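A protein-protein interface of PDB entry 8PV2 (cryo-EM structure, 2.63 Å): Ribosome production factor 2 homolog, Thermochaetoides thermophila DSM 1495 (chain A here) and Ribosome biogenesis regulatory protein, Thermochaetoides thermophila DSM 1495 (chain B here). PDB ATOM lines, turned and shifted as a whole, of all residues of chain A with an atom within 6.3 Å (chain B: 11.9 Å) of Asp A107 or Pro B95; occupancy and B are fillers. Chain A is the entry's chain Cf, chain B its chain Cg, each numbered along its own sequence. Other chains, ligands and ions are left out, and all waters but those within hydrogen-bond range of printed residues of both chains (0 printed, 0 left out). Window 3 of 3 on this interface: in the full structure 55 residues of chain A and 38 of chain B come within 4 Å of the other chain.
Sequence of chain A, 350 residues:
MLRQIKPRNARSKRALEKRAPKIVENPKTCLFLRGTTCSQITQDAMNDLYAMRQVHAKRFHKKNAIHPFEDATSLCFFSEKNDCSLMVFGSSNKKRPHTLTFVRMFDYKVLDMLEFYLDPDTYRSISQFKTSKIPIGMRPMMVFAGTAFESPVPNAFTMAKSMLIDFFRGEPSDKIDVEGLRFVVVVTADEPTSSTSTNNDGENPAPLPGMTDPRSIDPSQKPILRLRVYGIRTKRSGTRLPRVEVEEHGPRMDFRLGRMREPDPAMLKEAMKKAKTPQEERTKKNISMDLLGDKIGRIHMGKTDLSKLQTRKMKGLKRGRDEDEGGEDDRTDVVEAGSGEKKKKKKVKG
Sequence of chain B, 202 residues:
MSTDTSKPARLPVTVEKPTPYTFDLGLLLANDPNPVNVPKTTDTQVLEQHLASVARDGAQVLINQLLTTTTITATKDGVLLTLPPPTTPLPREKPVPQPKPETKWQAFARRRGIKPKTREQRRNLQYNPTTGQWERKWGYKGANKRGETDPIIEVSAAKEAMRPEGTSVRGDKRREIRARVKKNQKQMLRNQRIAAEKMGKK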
ATOM      1  N   PRO A  21     -25.671  -3.608  14.274  1.00  0.00           N
ATOM      2  CA  PRO A  21     -25.542  -4.677  13.277  1.00  0.00           C
ATOM      3  C   PRO A  21     -25.377  -4.123  11.870  1.00  0.00           C
ATOM      4  O   PRO A  21     -25.991  -3.120  11.500  1.00  0.00           O
ATOM      5  CB  PRO A  21     -26.855  -5.452  13.421  1.00  0.00           C
ATOM      6  CG  PRO A  21     -27.295  -5.176  14.806  1.00  0.00           C
ATOM      7  CD  PRO A  21     -26.894  -3.762  15.079  1.00  0.00           C
ATOM      8  N   LYS A  22     -24.548  -4.797  11.077  1.00  0.00           N
ATOM      9  CA  LYS A  22     -24.209  -4.338   9.739  1.00  0.00           C
ATOM     10  C   LYS A  22     -24.321  -5.491   8.756  1.00  0.00           C
ATOM     11  O   LYS A  22     -24.276  -6.664   9.133  1.00  0.00           O
ATOM     12  CB  LYS A  22     -22.794  -3.743   9.681  1.00  0.00           C
ATOM     13  CG  LYS A  22     -22.588  -2.522  10.558  1.00  0.00           C
ATOM     14  CD  LYS A  22     -21.122  -2.161  10.668  1.00  0.00           C
ATOM     15  CE  LYS A  22     -20.927  -0.975  11.591  1.00  0.00           C
ATOM     16  NZ  LYS A  22     -19.491  -0.618  11.735  1.00  0.00           N
ATOM     17  N   GLU A  25     -20.005  -7.213   8.402  1.00  0.00           N
ATOM     18  CA  GLU A  25     -19.678  -7.078   9.809  1.00  0.00           C
ATOM     19  C   GLU A  25     -18.216  -6.700  10.008  1.00  0.00           C
ATOM     20  O   GLU A  25     -17.348  -6.978   9.177  1.00  0.00           O
ATOM     21  CB  GLU A  25     -19.986  -8.371  10.556  1.00  0.00           C
ATOM     22  CG  GLU A  25     -21.457  -8.591  10.797  1.00  0.00           C
ATOM     23  CD  GLU A  25     -21.723  -9.792  11.664  1.00  0.00           C
ATOM     24  OE1 GLU A  25     -20.930 -10.754  11.607  1.00  0.00           O
ATOM     25  OE2 GLU A  25     -22.718  -9.770  12.416  1.00  0.00           O
ATOM     26  N   MET A 105     -20.003 -16.228  20.554  1.00  0.00           N
ATOM     27  CA  MET A 105     -21.354 -15.758  20.798  1.00  0.00           C
ATOM     28  C   MET A 105     -21.972 -15.062  19.598  1.00  0.00           C
ATOM     29  O   MET A 105     -21.280 -14.596  18.692  1.00  0.00           O
ATOM     30  CB  MET A 105     -21.427 -14.827  21.988  1.00  0.00           C
ATOM     31  CG  MET A 105     -20.742 -15.321  23.210  1.00  0.00           C
ATOM     32  SD  MET A 105     -20.780 -13.959  24.333  1.00  0.00           S
ATOM     33  CE  MET A 105     -21.154 -14.795  25.853  1.00  0.00           C
ATOM     34  N   PHE A 106     -23.299 -15.008  19.627  1.00  0.00           N
ATOM     35  CA  PHE A 106     -24.124 -14.412  18.591  1.00  0.00           C
ATOM     36  C   PHE A 106     -25.172 -13.547  19.273  1.00  0.00           C
ATOM     37  O   PHE A 106     -25.952 -14.057  20.081  1.00  0.00           O
ATOM     38  CB  PHE A 106     -24.789 -15.502  17.744  1.00  0.00           C
ATOM     39  CG  PHE A 106     -25.783 -14.984  16.752  1.00  0.00           C
ATOM     40  CD1 PHE A 106     -25.361 -14.366  15.592  1.00  0.00           C
ATOM     41  CD2 PHE A 106     -27.140 -15.118  16.979  1.00  0.00           C
ATOM     42  CE1 PHE A 106     -26.273 -13.891  14.679  1.00  0.00           C
ATOM     43  CE2 PHE A 106     -28.054 -14.644  16.070  1.00  0.00           C
ATOM     44  CZ  PHE A 106     -27.620 -14.029  14.919  1.00  0.00           C
ATOM     45  N   ASP A 107     -25.177 -12.248  18.952  1.00  0.00           N
ATOM     46  CA  ASP A 107     -26.113 -11.269  19.520  1.00  0.00           C
ATOM     47  C   ASP A 107     -26.057 -11.236  21.047  1.00  0.00           C
ATOM     48  O   ASP A 107     -27.087 -11.234  21.725  1.00  0.00           O
ATOM     49  CB  ASP A 107     -27.540 -11.523  19.034  1.00  0.00           C
ATOM     50  CG  ASP A 107     -28.400 -10.278  19.081  1.00  0.00           C
ATOM     51  OD1 ASP A 107     -27.854  -9.188  19.346  1.00  0.00           O
ATOM     52  OD2 ASP A 107     -29.622 -10.390  18.855  1.00  0.00           O
ATOM     53  N   TYR A 108     -24.833 -11.230  21.585  1.00  0.00           N
ATOM     54  CA  TYR A 108     -24.547 -11.137  23.024  1.00  0.00           C
ATOM     55  C   TYR A 108     -25.148 -12.295  23.816  1.00  0.00           C
ATOM     56  O   TYR A 108     -25.408 -12.171  25.013  1.00  0.00           O
ATOM     57  CB  TYR A 108     -25.002  -9.795  23.607  1.00  0.00           C
ATOM     58  CG  TYR A 108     -24.584  -8.610  22.774  1.00  0.00           C
ATOM     59  CD1 TYR A 108     -23.255  -8.418  22.429  1.00  0.00           C
ATOM     60  CD2 TYR A 108     -25.516  -7.685  22.337  1.00  0.00           C
ATOM     61  CE1 TYR A 108     -22.868  -7.342  21.662  1.00  0.00           C
ATOM     62  CE2 TYR A 108     -25.138  -6.604  21.572  1.00  0.00           C
ATOM     63  CZ  TYR A 108     -23.812  -6.437  21.238  1.00  0.00           C
ATOM     64  OH  TYR A 108     -23.431  -5.358  20.479  1.00  0.00           O
ATOM     65  N   LYS A 109     -25.375 -13.425  23.154  1.00  0.00           N
ATOM     66  CA  LYS A 109     -25.799 -14.656  23.801  1.00  0.00           C
ATOM     67  C   LYS A 109     -24.895 -15.775  23.317  1.00  0.00           C
ATOM     68  O   LYS A 109     -24.438 -15.758  22.173  1.00  0.00           O
ATOM     69  CB  LYS A 109     -27.261 -15.000  23.494  1.00  0.00           C
ATOM     70  CG  LYS A 109     -28.242 -13.899  23.815  1.00  0.00           C
ATOM     71  CD  LYS A 109     -29.564 -14.132  23.119  1.00  0.00           C
ATOM     72  CE  LYS A 109     -30.464 -12.916  23.241  1.00  0.00           C
ATOM     73  NZ  LYS A 109     -31.731 -13.081  22.481  1.00  0.00           N
ATOM     74  N   MET A 267     -30.967 -20.662  16.581  1.00  0.00           N
ATOM     75  CA  MET A 267     -29.930 -19.652  16.758  1.00  0.00           C
ATOM     76  C   MET A 267     -28.794 -19.857  15.767  1.00  0.00           C
ATOM     77  O   MET A 267     -28.246 -18.890  15.228  1.00  0.00           O
ATOM     78  CB  MET A 267     -29.415 -19.712  18.194  1.00  0.00           C
ATOM     79  CG  MET A 267     -28.226 -18.836  18.507  1.00  0.00           C
ATOM     80  SD  MET A 267     -28.059 -18.615  20.286  1.00  0.00           S
ATOM     81  CE  MET A 267     -27.147 -17.082  20.352  1.00  0.00           C
ATOM     82  N   GLU A 270     -29.950 -18.656  12.337  1.00  0.00           N
ATOM     83  CA  GLU A 270     -29.857 -17.199  12.302  1.00  0.00           C
ATOM     84  C   GLU A 270     -28.415 -16.720  12.202  1.00  0.00           C
ATOM     85  O   GLU A 270     -28.140 -15.737  11.506  1.00  0.00           O
ATOM     86  CB  GLU A 270     -30.519 -16.599  13.540  1.00  0.00           C
ATOM     87  CG  GLU A 270     -32.027 -16.736  13.566  1.00  0.00           C
ATOM     88  CD  GLU A 270     -32.700 -15.987  12.434  1.00  0.00           C
ATOM     89  OE1 GLU A 270     -33.700 -16.504  11.890  1.00  0.00           O
ATOM     90  OE2 GLU A 270     -32.238 -14.879  12.092  1.00  0.00           O
ATOM     91  N   LEU B  90     -18.731 -19.349   8.183  1.00  0.00           N
ATOM     92  CA  LEU B  90     -18.395 -18.941   9.537  1.00  0.00           C
ATOM     93  C   LEU B  90     -19.553 -18.142  10.112  1.00  0.00           C
ATOM     94  O   LEU B  90     -20.207 -17.385   9.385  1.00  0.00           O
ATOM     95  CB  LEU B  90     -17.107 -18.104   9.565  1.00  0.00           C
ATOM     96  CG  LEU B  90     -15.828 -18.886   9.266  1.00  0.00           C
ATOM     97  CD1 LEU B  90     -14.709 -17.957   8.858  1.00  0.00           C
ATOM     98  CD2 LEU B  90     -15.420 -19.700  10.472  1.00  0.00           C
ATOM     99  N   PRO B  91     -19.842 -18.301  11.403  1.00  0.00           N
ATOM    100  CA  PRO B  91     -21.012 -17.630  11.985  1.00  0.00           C
ATOM    101  C   PRO B  91     -20.824 -16.125  12.104  1.00  0.00           C
ATOM    102  O   PRO B  91     -19.709 -15.627  12.268  1.00  0.00           O
ATOM    103  CB  PRO B  91     -21.142 -18.284  13.364  1.00  0.00           C
ATOM    104  CG  PRO B  91     -19.783 -18.771  13.674  1.00  0.00           C
ATOM    105  CD  PRO B  91     -19.188 -19.195  12.372  1.00  0.00           C
ATOM    106  N   ARG B  92     -21.938 -15.405  12.021  1.00  0.00           N
ATOM    107  CA  ARG B  92     -21.947 -13.970  12.232  1.00  0.00           C
ATOM    108  C   ARG B  92     -21.927 -13.659  13.722  1.00  0.00           C
ATOM    109  O   ARG B  92     -22.255 -14.498  14.562  1.00  0.00           O
ATOM    110  CB  ARG B  92     -23.183 -13.335  11.602  1.00  0.00           C
ATOM    111  CG  ARG B  92     -23.169 -13.286  10.097  1.00  0.00           C
ATOM    112  CD  ARG B  92     -24.496 -12.787   9.573  1.00  0.00           C
ATOM    113  NE  ARG B  92     -24.861 -11.506  10.161  1.00  0.00           N
ATOM    114  CZ  ARG B  92     -24.577 -10.331   9.620  1.00  0.00           C
ATOM    115  NH1 ARG B  92     -23.932 -10.238   8.470  1.00  0.00           N
ATOM    116  NH2 ARG B  92     -24.947  -9.222  10.250  1.00  0.00           N
ATOM    117  N   GLU B  93     -21.541 -12.429  14.047  1.00  0.00           N
ATOM    118  CA  GLU B  93     -21.547 -11.998  15.437  1.00  0.00           C
ATOM    119  C   GLU B  93     -22.858 -11.340  15.839  1.00  0.00           C
ATOM    120  O   GLU B  93     -23.223 -11.376  17.019  1.00  0.00           O
ATOM    121  CB  GLU B  93     -20.379 -11.041  15.697  1.00  0.00           C
ATOM    122  CG  GLU B  93     -20.422  -9.754  14.903  1.00  0.00           C
ATOM    123  CD  GLU B  93     -19.198  -8.895  15.115  1.00  0.00           C
ATOM    124  OE1 GLU B  93     -18.308  -9.309  15.884  1.00  0.00           O
ATOM    125  OE2 GLU B  93     -19.122  -7.805  14.512  1.00  0.00           O
ATOM    126  N   LYS B  94     -23.573 -10.754  14.888  1.00  0.00           N
ATOM    127  CA  LYS B  94     -24.848 -10.091  15.091  1.00  0.00           C
ATOM    128  C   LYS B  94     -25.807 -10.509  13.988  1.00  0.00           C
ATOM    129  O   LYS B  94     -25.368 -10.889  12.899  1.00  0.00           O
ATOM    130  CB  LYS B  94     -24.679  -8.565  15.089  1.00  0.00           C
ATOM    131  CG  LYS B  94     -23.938  -8.027  16.291  1.00  0.00           C
ATOM    132  CD  LYS B  94     -23.421  -6.633  16.030  1.00  0.00           C
ATOM    133  CE  LYS B  94     -22.454  -6.197  17.109  1.00  0.00           C
ATOM    134  NZ  LYS B  94     -21.789  -4.917  16.751  1.00  0.00           N
ATOM    135  N   PRO B  95     -27.116 -10.468  14.242  1.00  0.00           N
ATOM    136  CA  PRO B  95     -28.075 -10.838  13.197  1.00  0.00           C
ATOM    137  C   PRO B  95     -28.077  -9.842  12.048  1.00  0.00           C
ATOM    138  O   PRO B  95     -27.618  -8.706  12.180  1.00  0.00           O
ATOM    139  CB  PRO B  95     -29.421 -10.842  13.930  1.00  0.00           C
ATOM    140  CG  PRO B  95     -29.195 -10.051  15.157  1.00  0.00           C
ATOM    141  CD  PRO B  95     -27.780 -10.286  15.542  1.00  0.00           C
ATOM    142  N   VAL B  96     -28.574 -10.304  10.903  1.00  0.00           N
ATOM    143  CA  VAL B  96     -28.673  -9.461   9.706  1.00  0.00           C
ATOM    144  C   VAL B  96     -29.624  -8.309   9.994  1.00  0.00           C
ATOM    145  O   VAL B  96     -30.668  -8.522  10.646  1.00  0.00           O
ATOM    146  CB  VAL B  96     -29.154 -10.296   8.506  1.00  0.00           C
ATOM    147  CG1 VAL B  96     -29.444  -9.426   7.297  1.00  0.00           C
ATOM    148  CG2 VAL B  96     -28.130 -11.354   8.156  1.00  0.00           C
ATOM    149  N   PRO B  97     -29.296  -7.073   9.610  1.00  0.00           N
ATOM    150  CA  PRO B  97     -30.210  -5.949   9.855  1.00  0.00           C
ATOM    151  C   PRO B  97     -31.543  -6.133   9.146  1.00  0.00           C
ATOM    152  O   PRO B  97     -31.604  -6.580   7.999  1.00  0.00           O
ATOM    153  CB  PRO B  97     -29.442  -4.744   9.304  1.00  0.00           C
ATOM    154  CG  PRO B  97     -28.021  -5.146   9.366  1.00  0.00           C
ATOM    155  CD  PRO B  97     -27.994  -6.617   9.097  1.00  0.00           C
ATOM    156  N   GLN B  98     -32.611  -5.777   9.842  1.00  0.00           N
ATOM    157  CA  GLN B  98     -33.976  -5.884   9.366  1.00  0.00           C
ATOM    158  C   GLN B  98     -34.569  -4.490   9.240  1.00  0.00           C
ATOM    159  O   GLN B  98     -34.097  -3.550   9.890  1.00  0.00           O
ATOM    160  CB  GLN B  98     -34.824  -6.729  10.328  1.00  0.00           C
ATOM    161  CG  GLN B  98     -34.371  -8.174  10.459  1.00  0.00           C
ATOM    162  CD  GLN B  98     -34.484  -8.942   9.158  1.00  0.00           C
ATOM    163  OE1 GLN B  98     -33.477  -9.295   8.542  1.00  0.00           O
ATOM    164  NE2 GLN B  98     -35.712  -9.208   8.732  1.00  0.00           N
ATOM    165  N   PRO B  99     -35.570  -4.307   8.378  1.00  0.00           N
ATOM    166  CA  PRO B  99     -36.262  -3.014   8.326  1.00  0.00           C
ATOM    167  C   PRO B  99     -36.935  -2.688   9.650  1.00  0.00           C
ATOM    168  O   PRO B  99     -37.483  -3.564  10.323  1.00  0.00           O
ATOM    169  CB  PRO B  99     -37.286  -3.206   7.204  1.00  0.00           C
ATOM    170  CG  PRO B  99     -36.698  -4.264   6.344  1.00  0.00           C
ATOM    171  CD  PRO B  99     -35.993  -5.196   7.281  1.00  0.00           C
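The guanidinium group (NH2) of Arg B92 is in salt-bridge range of the side-chain carboxylate (OE2) of Glu A25 (3.2 Å).
OE1 of Glu A25 is in hydrogen-bond range of N of Glu B93 (3.0 Å).
The backbone NH (N) of Asp A107 is in hydrogen-bond range of the backbone carbonyl oxygen (O) of Glu B93.
The side-chain carboxylate (OE2) of Glu A25 is in hydrogen-bond range of the backbone NH (N) of Lys B94 (2.8 Å).
O of Lys A22 sits at hydrogen-bond distance from NH2 of Arg B92, 2.9 Å away.
NH2 of Arg B92 lies within hydrogen-bond range of O of Pro B95 (3.3 Å).
The guanidinium group (NE) of Arg B92 is in hydrogen-bond range of the backbone carbonyl oxygen (O) of Lys B94, 2.9 Å away.
Pro A21 touches Lys B94.
O of Pro B95 touches CB of Pro A21, 3.6 Å away.
Pro A21 touches Pro B97.
Lys A22 touches Pro B97 (O to CD, 3.7 Å).
CD1 of Phe A106 touches O of Arg B92 (3.3 Å).
Glu B93 touches Phe A106.
CE1 of Phe A106 touches C of Lys B94, 3.5 Å away.
Pro B95 touches Phe A106 (N to CE1, 3.6 Å).
Asp A107 touches Pro B95.
OH of Tyr A108 touches CE of Lys B94 (3.6 Å).
Asp A107 touches just these residues of chain B: Glu B93 (2.9 Å) and Pro B95 (3.6 Å).
Of chain B, only Lys B94 (3.6 Å) comes within 4 Å of Tyr A108.
Of the printed residues of chain A, Arg B92 touches Lys A22, Glu A25 and Phe A106.
Of the printed residues of chain B, Pro A21 touches Lys B94 (3.99 Å), Pro B95 (3.6 Å) and Pro B97 (3.6 Å).
Glu A270 touches none of the printed residues of chain B.
The nearest residue of chain B that does not touch Asp A107 is Lys B94 (4.4 Å).
The nearest printed residue of chain B that does not touch Glu A25 is Pro B95 (4.8 Å).
Hydrophobic or aromatic side chains of chain A within 4 Å of the printed part of chain B: Pro A21, Phe A106 and Tyr A108.
Of the 10 printed residues of chain B, 5 touch a printed residue of chain A.
Among the printed residues, 15 pairs touch across the chains.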
